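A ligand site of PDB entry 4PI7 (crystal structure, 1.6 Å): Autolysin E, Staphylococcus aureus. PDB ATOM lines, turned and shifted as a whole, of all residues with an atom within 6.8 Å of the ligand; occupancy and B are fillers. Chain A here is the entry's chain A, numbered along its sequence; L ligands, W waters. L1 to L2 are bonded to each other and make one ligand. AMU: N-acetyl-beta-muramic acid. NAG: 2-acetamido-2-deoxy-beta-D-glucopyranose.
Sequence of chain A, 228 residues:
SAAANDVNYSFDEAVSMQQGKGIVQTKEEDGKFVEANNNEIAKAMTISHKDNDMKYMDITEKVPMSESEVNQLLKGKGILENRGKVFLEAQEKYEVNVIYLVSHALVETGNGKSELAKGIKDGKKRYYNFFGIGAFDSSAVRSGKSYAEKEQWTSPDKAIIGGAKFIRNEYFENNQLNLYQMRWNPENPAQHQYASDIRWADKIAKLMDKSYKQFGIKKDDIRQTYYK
An oxygen (O10) of AMU L1 lies within hydrogen-bond range of the side-chain hydroxyl (OH) of Tyr 171, 2.7 Å away.
The backbone NH (N) of Gly 134 is in hydrogen-bond range of an oxygen (O7) of AMU L1, at 2.8 Å.
O of Tyr 194 sits at hydrogen-bond distance from N2 of AMU L1 (2.8 Å).
The backbone NH of Gln 193 sits at hydrogen-bond distance from an oxygen (O7) of NAG L2, 2.9 Å away.
N of His 192 lies within hydrogen-bond range of O7 of NAG L2 (3.1 Å).
The backbone carbonyl oxygen (O) of Phe 131 lies within hydrogen-bond range of the side-chain hydroxyl (OH) of Tyr 194, 2.7 Å away.
OE1 of Gln 193 is in hydrogen-bond range of N of Ala 190.
The side-chain amide oxygen (OE1) of Gln 193 lies within hydrogen-bond range of the side-chain amide nitrogen (NE2) of Gln 18, at 2.8 Å.
NE2 of Gln 193 sits close to O of Arg 183.
The side-chain amide nitrogen (NE2) of Gln 18 lies close to the backbone NH (N) of Ala 190.
The guanidinium group (NH2) of Arg 183 is in hydrogen-bond range of the backbone carbonyl oxygen (O) of Ser 196, 2.9 Å away.
O of Gly 132 touches C7 of AMU L1 (3.4 Å).
Ile 133 touches the ligand.
CZ of Phe 166 touches O10 of AMU L1, 3.6 Å away.
O of Ala 190 touches C8 of NAG L2, at 3.3 Å.
Gln 191 touches the ligand.
Ser 196 touches the ligand.
Within 4 Å of the ligand: Gly 132, Ile 133, Gly 134, Phe 166, Tyr 171, Ala 190, Gln 191, His 192, Gln 193, Tyr 194 and Ser 196.
Water W9 lies within hydrogen-bond range of a ring nitrogen (NE2) of His 192 (2.7 Å) and an oxygen (O10) of AMU L1 (2.8 Å).
Water W2 lies within hydrogen-bond range of the backbone carbonyl oxygen of Ala 190 (2.7 Å) and an oxygen (O3) of NAG L2 (2.8 Å).
Water W4 lies within hydrogen-bond range of an oxygen (O3) of NAG L2 (2.9 Å) and the backbone NH of His 192 (3.0 Å).
Water W7 lies within hydrogen-bond range of O of Gly 134 (2.9 Å), O1 of AMU L1 (2.9 Å) and O of Gly 132 (3.0 Å).
Water W1 bridges the backbone carbonyl oxygen of Val 24 (2.7 Å) and an oxygen (O6) of AMU L1 (2.9 Å).
Water W10 lies within hydrogen-bond range of the backbone carbonyl oxygen of Tyr 194 (2.9 Å), the backbone carbonyl oxygen of Gly 132 (2.9 Å) and an oxygen (O1) of AMU L1 (3.1 Å).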
ATOM      1  N   GLN A  18      34.288  38.484 -14.215  1.00  0.00           N
ATOM      2  CA  GLN A  18      33.260  38.337 -15.284  1.00  0.00           C
ATOM      3  C   GLN A  18      33.675  39.069 -16.563  1.00  0.00           C
ATOM      4  O   GLN A  18      33.271  38.682 -17.639  1.00  0.00           O
ATOM      5  CB  GLN A  18      31.918  38.888 -14.817  1.00  0.00           C
ATOM      6  CG  GLN A  18      31.299  38.204 -13.634  1.00  0.00           C
ATOM      7  CD  GLN A  18      30.773  36.826 -13.928  1.00  0.00           C
ATOM      8  OE1 GLN A  18      30.734  36.372 -15.048  1.00  0.00           O
ATOM      9  NE2 GLN A  18      30.349  36.160 -12.888  1.00  0.00           N
ATOM     10  N   ILE A  23      35.789  35.788 -21.995  1.00  0.00           N
ATOM     11  CA  ILE A  23      34.561  35.296 -21.422  1.00  0.00           C
ATOM     12  C   ILE A  23      33.417  35.921 -22.206  1.00  0.00           C
ATOM     13  O   ILE A  23      33.310  37.154 -22.271  1.00  0.00           O
ATOM     14  CB  ILE A  23      34.464  35.634 -19.954  1.00  0.00           C
ATOM     15  CG1 ILE A  23      35.565  34.842 -19.199  1.00  0.00           C
ATOM     16  CG2 ILE A  23      33.093  35.301 -19.384  1.00  0.00           C
ATOM     17  CD1 ILE A  23      35.862  35.429 -17.850  1.00  0.00           C
ATOM     18  N   VAL A  24      32.567  35.048 -22.735  1.00  0.00           N
ATOM     19  CA  VAL A  24      31.424  35.519 -23.540  1.00  0.00           C
ATOM     20  C   VAL A  24      30.267  36.031 -22.663  1.00  0.00           C
ATOM     21  O   VAL A  24      29.714  35.274 -21.862  1.00  0.00           O
ATOM     22  CB  VAL A  24      30.946  34.405 -24.459  1.00  0.00           C
ATOM     23  CG1 VAL A  24      29.792  34.911 -25.327  1.00  0.00           C
ATOM     24  CG2 VAL A  24      32.118  33.890 -25.298  1.00  0.00           C
ATOM     25  N   GLN A  25      29.939  37.308 -22.817  1.00  0.00           N
ATOM     26  CA  GLN A  25      28.828  37.932 -22.119  1.00  0.00           C
ATOM     27  C   GLN A  25      28.084  38.672 -23.223  1.00  0.00           C
ATOM     28  O   GLN A  25      28.683  39.495 -23.883  1.00  0.00           O
ATOM     29  CB  GLN A  25      29.261  38.864 -21.012  1.00  0.00           C
ATOM     30  CG  GLN A  25      30.367  38.277 -20.093  1.00  0.00           C
ATOM     31  CD  GLN A  25      29.875  37.640 -18.801  1.00  0.00           C
ATOM     32  OE1 GLN A  25      30.644  37.437 -17.829  1.00  0.00           O
ATOM     33  NE2 GLN A  25      28.687  37.245 -18.792  1.00  0.00           N
ATOM     34  N   PHE A 131      16.379  23.426 -22.971  1.00  0.00           N
ATOM     35  CA  PHE A 131      16.998  24.215 -21.910  1.00  0.00           C
ATOM     36  C   PHE A 131      18.366  24.773 -22.235  1.00  0.00           C
ATOM     37  O   PHE A 131      19.125  25.153 -21.305  1.00  0.00           O
ATOM     38  CB  PHE A 131      17.016  23.415 -20.579  1.00  0.00           C
ATOM     39  CG  PHE A 131      15.641  22.977 -20.126  1.00  0.00           C
ATOM     40  CD1 PHE A 131      14.788  23.802 -19.418  1.00  0.00           C
ATOM     41  CD2 PHE A 131      15.191  21.721 -20.482  1.00  0.00           C
ATOM     42  CE1 PHE A 131      13.500  23.394 -19.065  1.00  0.00           C
ATOM     43  CE2 PHE A 131      13.974  21.280 -20.081  1.00  0.00           C
ATOM     44  CZ  PHE A 131      13.092  22.109 -19.417  1.00  0.00           C
ATOM     45  N   GLY A 132      18.715  24.787 -23.509  1.00  0.00           N
ATOM     46  CA  GLY A 132      20.020  25.372 -23.864  1.00  0.00           C
ATOM     47  C   GLY A 132      21.208  24.681 -23.276  1.00  0.00           C
ATOM     48  O   GLY A 132      22.185  25.344 -22.916  1.00  0.00           O
ATOM     49  N   ILE A 133      21.178  23.352 -23.205  1.00  0.00           N
ATOM     50  CA  ILE A 133      22.175  22.533 -22.572  1.00  0.00           C
ATOM     51  C   ILE A 133      23.153  22.013 -23.613  1.00  0.00           C
ATOM     52  O   ILE A 133      22.809  21.192 -24.489  1.00  0.00           O
ATOM     53  CB  ILE A 133      21.557  21.366 -21.772  1.00  0.00           C
ATOM     54  CG1 ILE A 133      20.627  21.912 -20.675  1.00  0.00           C
ATOM     55  CG2 ILE A 133      22.630  20.513 -21.141  1.00  0.00           C
ATOM     56  CD1 ILE A 133      19.667  20.886 -20.129  1.00  0.00           C
ATOM     57  N   GLY A 134      24.400  22.491 -23.491  1.00  0.00           N
ATOM     58  CA  GLY A 134      25.488  22.026 -24.343  1.00  0.00           C
ATOM     59  C   GLY A 134      25.333  22.460 -25.775  1.00  0.00           C
ATOM     60  O   GLY A 134      24.570  23.380 -26.086  1.00  0.00           O
ATOM     61  N   ALA A 135      26.113  21.829 -26.658  1.00  0.00           N
ATOM     62  CA  ALA A 135      26.114  22.188 -28.051  1.00  0.00           C
ATOM     63  C   ALA A 135      24.929  21.516 -28.712  1.00  0.00           C
ATOM     64  O   ALA A 135      24.767  20.292 -28.564  1.00  0.00           O
ATOM     65  CB  ALA A 135      27.430  21.732 -28.727  1.00  0.00           C
ATOM     66  N   PHE A 166      19.489  17.293 -15.505  1.00  0.00           N
ATOM     67  CA  PHE A 166      20.730  18.036 -15.681  1.00  0.00           C
ATOM     68  C   PHE A 166      20.769  19.225 -14.703  1.00  0.00           C
ATOM     69  O   PHE A 166      21.785  19.472 -14.011  1.00  0.00           O
ATOM     70  CB  PHE A 166      20.829  18.552 -17.110  1.00  0.00           C
ATOM     71  CG  PHE A 166      21.995  19.477 -17.325  1.00  0.00           C
ATOM     72  CD1 PHE A 166      23.247  18.963 -17.620  1.00  0.00           C
ATOM     73  CD2 PHE A 166      21.818  20.824 -17.316  1.00  0.00           C
ATOM     74  CE1 PHE A 166      24.335  19.804 -17.840  1.00  0.00           C
ATOM     75  CE2 PHE A 166      22.889  21.669 -17.550  1.00  0.00           C
ATOM     76  CZ  PHE A 166      24.143  21.153 -17.812  1.00  0.00           C
ATOM     77  N   GLU A 170      23.635  19.115 -11.987  1.00  0.00           N
ATOM     78  CA  GLU A 170      24.804  19.904 -12.322  1.00  0.00           C
ATOM     79  C   GLU A 170      24.785  21.292 -11.711  1.00  0.00           C
ATOM     80  O   GLU A 170      25.850  21.847 -11.430  1.00  0.00           O
ATOM     81  CB  GLU A 170      25.028  19.978 -13.829  1.00  0.00           C
ATOM     82  CG  GLU A 170      25.096  18.616 -14.466  1.00  0.00           C
ATOM     83  CD  GLU A 170      26.134  17.735 -13.829  1.00  0.00           C
ATOM     84  OE1 GLU A 170      27.263  18.237 -13.563  1.00  0.00           O
ATOM     85  OE2 GLU A 170      25.823  16.533 -13.592  1.00  0.00           O
ATOM     86  N   TYR A 171      23.601  21.864 -11.484  1.00  0.00           N
ATOM     87  CA  TYR A 171      23.477  23.162 -10.868  1.00  0.00           C
ATOM     88  C   TYR A 171      22.995  23.104  -9.420  1.00  0.00           C
ATOM     89  O   TYR A 171      23.681  23.620  -8.499  1.00  0.00           O
ATOM     90  CB  TYR A 171      22.607  24.126 -11.762  1.00  0.00           C
ATOM     91  CG  TYR A 171      23.424  24.597 -12.953  1.00  0.00           C
ATOM     92  CD1 TYR A 171      23.585  23.781 -14.064  1.00  0.00           C
ATOM     93  CD2 TYR A 171      24.096  25.817 -12.946  1.00  0.00           C
ATOM     94  CE1 TYR A 171      24.349  24.171 -15.130  1.00  0.00           C
ATOM     95  CE2 TYR A 171      24.896  26.182 -13.992  1.00  0.00           C
ATOM     96  CZ  TYR A 171      25.024  25.362 -15.078  1.00  0.00           C
ATOM     97  OH  TYR A 171      25.839  25.769 -16.115  1.00  0.00           O
ATOM     98  N   ARG A 183      23.428  31.950 -13.092  1.00  0.00           N
ATOM     99  CA  ARG A 183      23.988  32.839 -14.104  1.00  0.00           C
ATOM    100  C   ARG A 183      25.329  33.425 -13.768  1.00  0.00           C
ATOM    101  O   ARG A 183      26.151  33.581 -14.643  1.00  0.00           O
ATOM    102  CB  ARG A 183      22.989  33.972 -14.390  1.00  0.00           C
ATOM    103  CG  ARG A 183      23.450  35.005 -15.386  1.00  0.00           C
ATOM    104  CD  ARG A 183      23.773  34.439 -16.739  1.00  0.00           C
ATOM    105  NE  ARG A 183      24.278  35.398 -17.700  1.00  0.00           N
ATOM    106  CZ  ARG A 183      25.541  35.813 -17.761  1.00  0.00           C
ATOM    107  NH1 ARG A 183      26.468  35.376 -16.889  1.00  0.00           N
ATOM    108  NH2 ARG A 183      25.902  36.689 -18.695  1.00  0.00           N
ATOM    109  N   ALA A 190      32.530  33.533 -12.914  1.00  0.00           N
ATOM    110  CA  ALA A 190      32.931  33.301 -14.289  1.00  0.00           C
ATOM    111  C   ALA A 190      33.180  31.832 -14.666  1.00  0.00           C
ATOM    112  O   ALA A 190      33.650  31.534 -15.783  1.00  0.00           O
ATOM    113  CB  ALA A 190      34.112  34.206 -14.715  1.00  0.00           C
ATOM    114  N   GLN A 191      32.911  30.910 -13.755  1.00  0.00           N
ATOM    115  CA  GLN A 191      32.920  29.489 -14.002  1.00  0.00           C
ATOM    116  C   GLN A 191      31.499  28.967 -13.883  1.00  0.00           C
ATOM    117  O   GLN A 191      30.735  29.417 -13.061  1.00  0.00           O
ATOM    118  CB  GLN A 191      33.741  28.757 -12.920  1.00  0.00           C
ATOM    119  CG  GLN A 191      35.200  29.082 -13.023  1.00  0.00           C
ATOM    120  CD  GLN A 191      36.030  28.130 -12.197  1.00  0.00           C
ATOM    121  OE1 GLN A 191      36.491  28.441 -11.083  1.00  0.00           O
ATOM    122  NE2 GLN A 191      36.144  26.947 -12.699  1.00  0.00           N
ATOM    123  N   HIS A 192      31.256  27.909 -14.660  1.00  0.00           N
ATOM    124  CA  HIS A 192      30.041  27.119 -14.571  1.00  0.00           C
ATOM    125  C   HIS A 192      28.765  27.967 -14.539  1.00  0.00           C
ATOM    126  O   HIS A 192      27.928  27.837 -13.624  1.00  0.00           O
ATOM    127  CB  HIS A 192      30.056  26.205 -13.361  1.00  0.00           C
ATOM    128  CG  HIS A 192      29.110  25.067 -13.512  1.00  0.00           C
ATOM    129  ND1 HIS A 192      27.930  24.967 -12.820  1.00  0.00           N
ATOM    130  CD2 HIS A 192      29.109  24.046 -14.412  1.00  0.00           C
ATOM    131  CE1 HIS A 192      27.281  23.890 -13.192  1.00  0.00           C
ATOM    132  NE2 HIS A 192      27.935  23.342 -14.206  1.00  0.00           N
ATOM    133  N   GLN A 193      28.665  28.852 -15.521  1.00  0.00           N
ATOM    134  CA  GLN A 193      27.510  29.743 -15.636  1.00  0.00           C
ATOM    135  C   GLN A 193      26.601  29.275 -16.736  1.00  0.00           C
ATOM    136  O   GLN A 193      27.025  28.862 -17.826  1.00  0.00           O
ATOM    137  CB  GLN A 193      28.008  31.168 -15.858  1.00  0.00           C
ATOM    138  CG  GLN A 193      28.666  31.665 -14.583  1.00  0.00           C
ATOM    139  CD  GLN A 193      29.291  33.063 -14.572  1.00  0.00           C
ATOM    140  OE1 GLN A 193      29.687  33.513 -13.469  1.00  0.00           O
ATOM    141  NE2 GLN A 193      29.405  33.756 -15.712  1.00  0.00           N
ATOM    142  N   TYR A 194      25.299  29.421 -16.491  1.00  0.00           N
ATOM    143  CA  TYR A 194      24.312  28.723 -17.347  1.00  0.00           C
ATOM    144  C   TYR A 194      24.218  29.311 -18.741  1.00  0.00           C
ATOM    145  O   TYR A 194      23.951  28.569 -19.707  1.00  0.00           O
ATOM    146  CB  TYR A 194      22.947  28.690 -16.660  1.00  0.00           C
ATOM    147  CG  TYR A 194      22.067  27.538 -17.207  1.00  0.00           C
ATOM    148  CD1 TYR A 194      21.402  27.695 -18.407  1.00  0.00           C
ATOM    149  CD2 TYR A 194      21.969  26.353 -16.530  1.00  0.00           C
ATOM    150  CE1 TYR A 194      20.670  26.656 -18.947  1.00  0.00           C
ATOM    151  CE2 TYR A 194      21.231  25.284 -17.078  1.00  0.00           C
ATOM    152  CZ  TYR A 194      20.613  25.478 -18.275  1.00  0.00           C
ATOM    153  OH  TYR A 194      19.872  24.401 -18.778  1.00  0.00           O
ATOM    154  N   ALA A 195      24.427  30.614 -18.883  1.00  0.00           N
ATOM    155  CA  ALA A 195      24.179  31.310 -20.108  1.00  0.00           C
ATOM    156  C   ALA A 195      25.087  32.527 -20.236  1.00  0.00           C
ATOM    157  O   ALA A 195      25.598  33.049 -19.220  1.00  0.00           O
ATOM    158  CB  ALA A 195      22.704  31.714 -20.165  1.00  0.00           C
ATOM    159  N   SER A 196      25.280  32.991 -21.484  1.00  0.00           N
ATOM    160  CA  SER A 196      26.026  34.196 -21.762  1.00  0.00           C
ATOM    161  C   SER A 196      25.171  35.444 -21.784  1.00  0.00           C
ATOM    162  O   SER A 196      25.655  36.518 -21.533  1.00  0.00           O
ATOM    163  CB  SER A 196      26.802  34.048 -23.073  1.00  0.00           C
ATOM    164  OG  SER A 196      25.959  34.076 -24.224  1.00  0.00           O
HETATM  165  C1  AMU L   1      26.122  28.288 -22.219  1.00  0.00           C
HETATM  166  C2  AMU L   1      26.413  26.893 -21.660  1.00  0.00           C
HETATM  167  C3  AMU L   1      27.619  27.019 -20.752  1.00  0.00           C
HETATM  168  C4  AMU L   1      28.785  27.687 -21.478  1.00  0.00           C
HETATM  169  C5  AMU L   1      28.363  28.988 -22.137  1.00  0.00           C
HETATM  170  C6  AMU L   1      29.496  29.580 -22.978  1.00  0.00           C
HETATM  171  C7  AMU L   1      24.888  25.095 -20.858  1.00  0.00           C
HETATM  172  C8  AMU L   1      23.782  24.857 -19.891  1.00  0.00           C
HETATM  173  C9  AMU L   1      27.703  25.519 -18.868  1.00  0.00           C
HETATM  174  C10 AMU L   1      27.452  24.069 -18.620  1.00  0.00           C
HETATM  175  C11 AMU L   1      28.847  26.031 -17.990  1.00  0.00           C
HETATM  176  O1  AMU L   1      25.005  28.273 -23.106  1.00  0.00           O
HETATM  177  O3  AMU L   1      28.031  25.740 -20.254  1.00  0.00           O
HETATM  178  O4  AMU L   1      29.770  27.926 -20.460  1.00  0.00           O
HETATM  179  O5  AMU L   1      27.250  28.719 -22.989  1.00  0.00           O
HETATM  180  O6  AMU L   1      29.085  30.834 -23.520  1.00  0.00           O
HETATM  181  O7  AMU L   1      25.350  24.213 -21.566  1.00  0.00           O
HETATM  182  O10 AMU L   1      26.678  23.725 -17.695  1.00  0.00           O
HETATM  183  O11 AMU L   1      28.020  23.166 -19.326  1.00  0.00           O
HETATM  184  N2  AMU L   1      25.306  26.344 -20.862  1.00  0.00           N
HETATM  185  C1  NAG L   2      31.065  27.533 -20.848  1.00  0.00           C
HETATM  186  C2  NAG L   2      31.978  28.040 -19.736  1.00  0.00           C
HETATM  187  C3  NAG L   2      33.400  27.582 -20.010  1.00  0.00           C
HETATM  188  C4  NAG L   2      33.417  26.103 -20.247  1.00  0.00           C
HETATM  189  C5  NAG L   2      32.426  25.664 -21.310  1.00  0.00           C
HETATM  190  C6  NAG L   2      32.342  24.155 -21.370  1.00  0.00           C
HETATM  191  C7  NAG L   2      31.335  29.963 -18.280  1.00  0.00           C
HETATM  192  C8  NAG L   2      31.391  31.455 -18.131  1.00  0.00           C
HETATM  193  N2  NAG L   2      31.899  29.464 -19.409  1.00  0.00           N
HETATM  194  O3  NAG L   2      34.178  27.846 -18.875  1.00  0.00           O
HETATM  195  O4  NAG L   2      34.733  25.775 -20.680  1.00  0.00           O
HETATM  196  O5  NAG L   2      31.146  26.108 -20.933  1.00  0.00           O
HETATM  197  O6  NAG L   2      31.437  23.922 -22.435  1.00  0.00           O
HETATM  198  O7  NAG L   2      30.824  29.217 -17.414  1.00  0.00           O
HETATM  199  O   HOH W   1      29.594  32.657 -21.258  1.00  0.00           O
HETATM  200  O   HOH W   2      34.971  30.315 -17.746  1.00  0.00           O
HETATM  201  O   HOH W   3      28.636  23.856 -22.051  1.00  0.00           O
HETATM  202  O   HOH W   4      33.309  26.594 -16.443  1.00  0.00           O
HETATM  203  O   HOH W   5      36.811  27.299 -19.481  1.00  0.00           O
HETATM  204  O   HOH W   6      28.114  31.004 -19.636  1.00  0.00           O
HETATM  205  O   HOH W   7      24.688  25.780 -24.514  1.00  0.00           O
HETATM  206  O   HOH W   8      30.492  22.461 -18.521  1.00  0.00           O
HETATM  207  O   HOH W   9      27.274  21.489 -16.071  1.00  0.00           O
HETATM  208  O   HOH W  10      22.104  28.081 -21.896  1.00  0.00           O
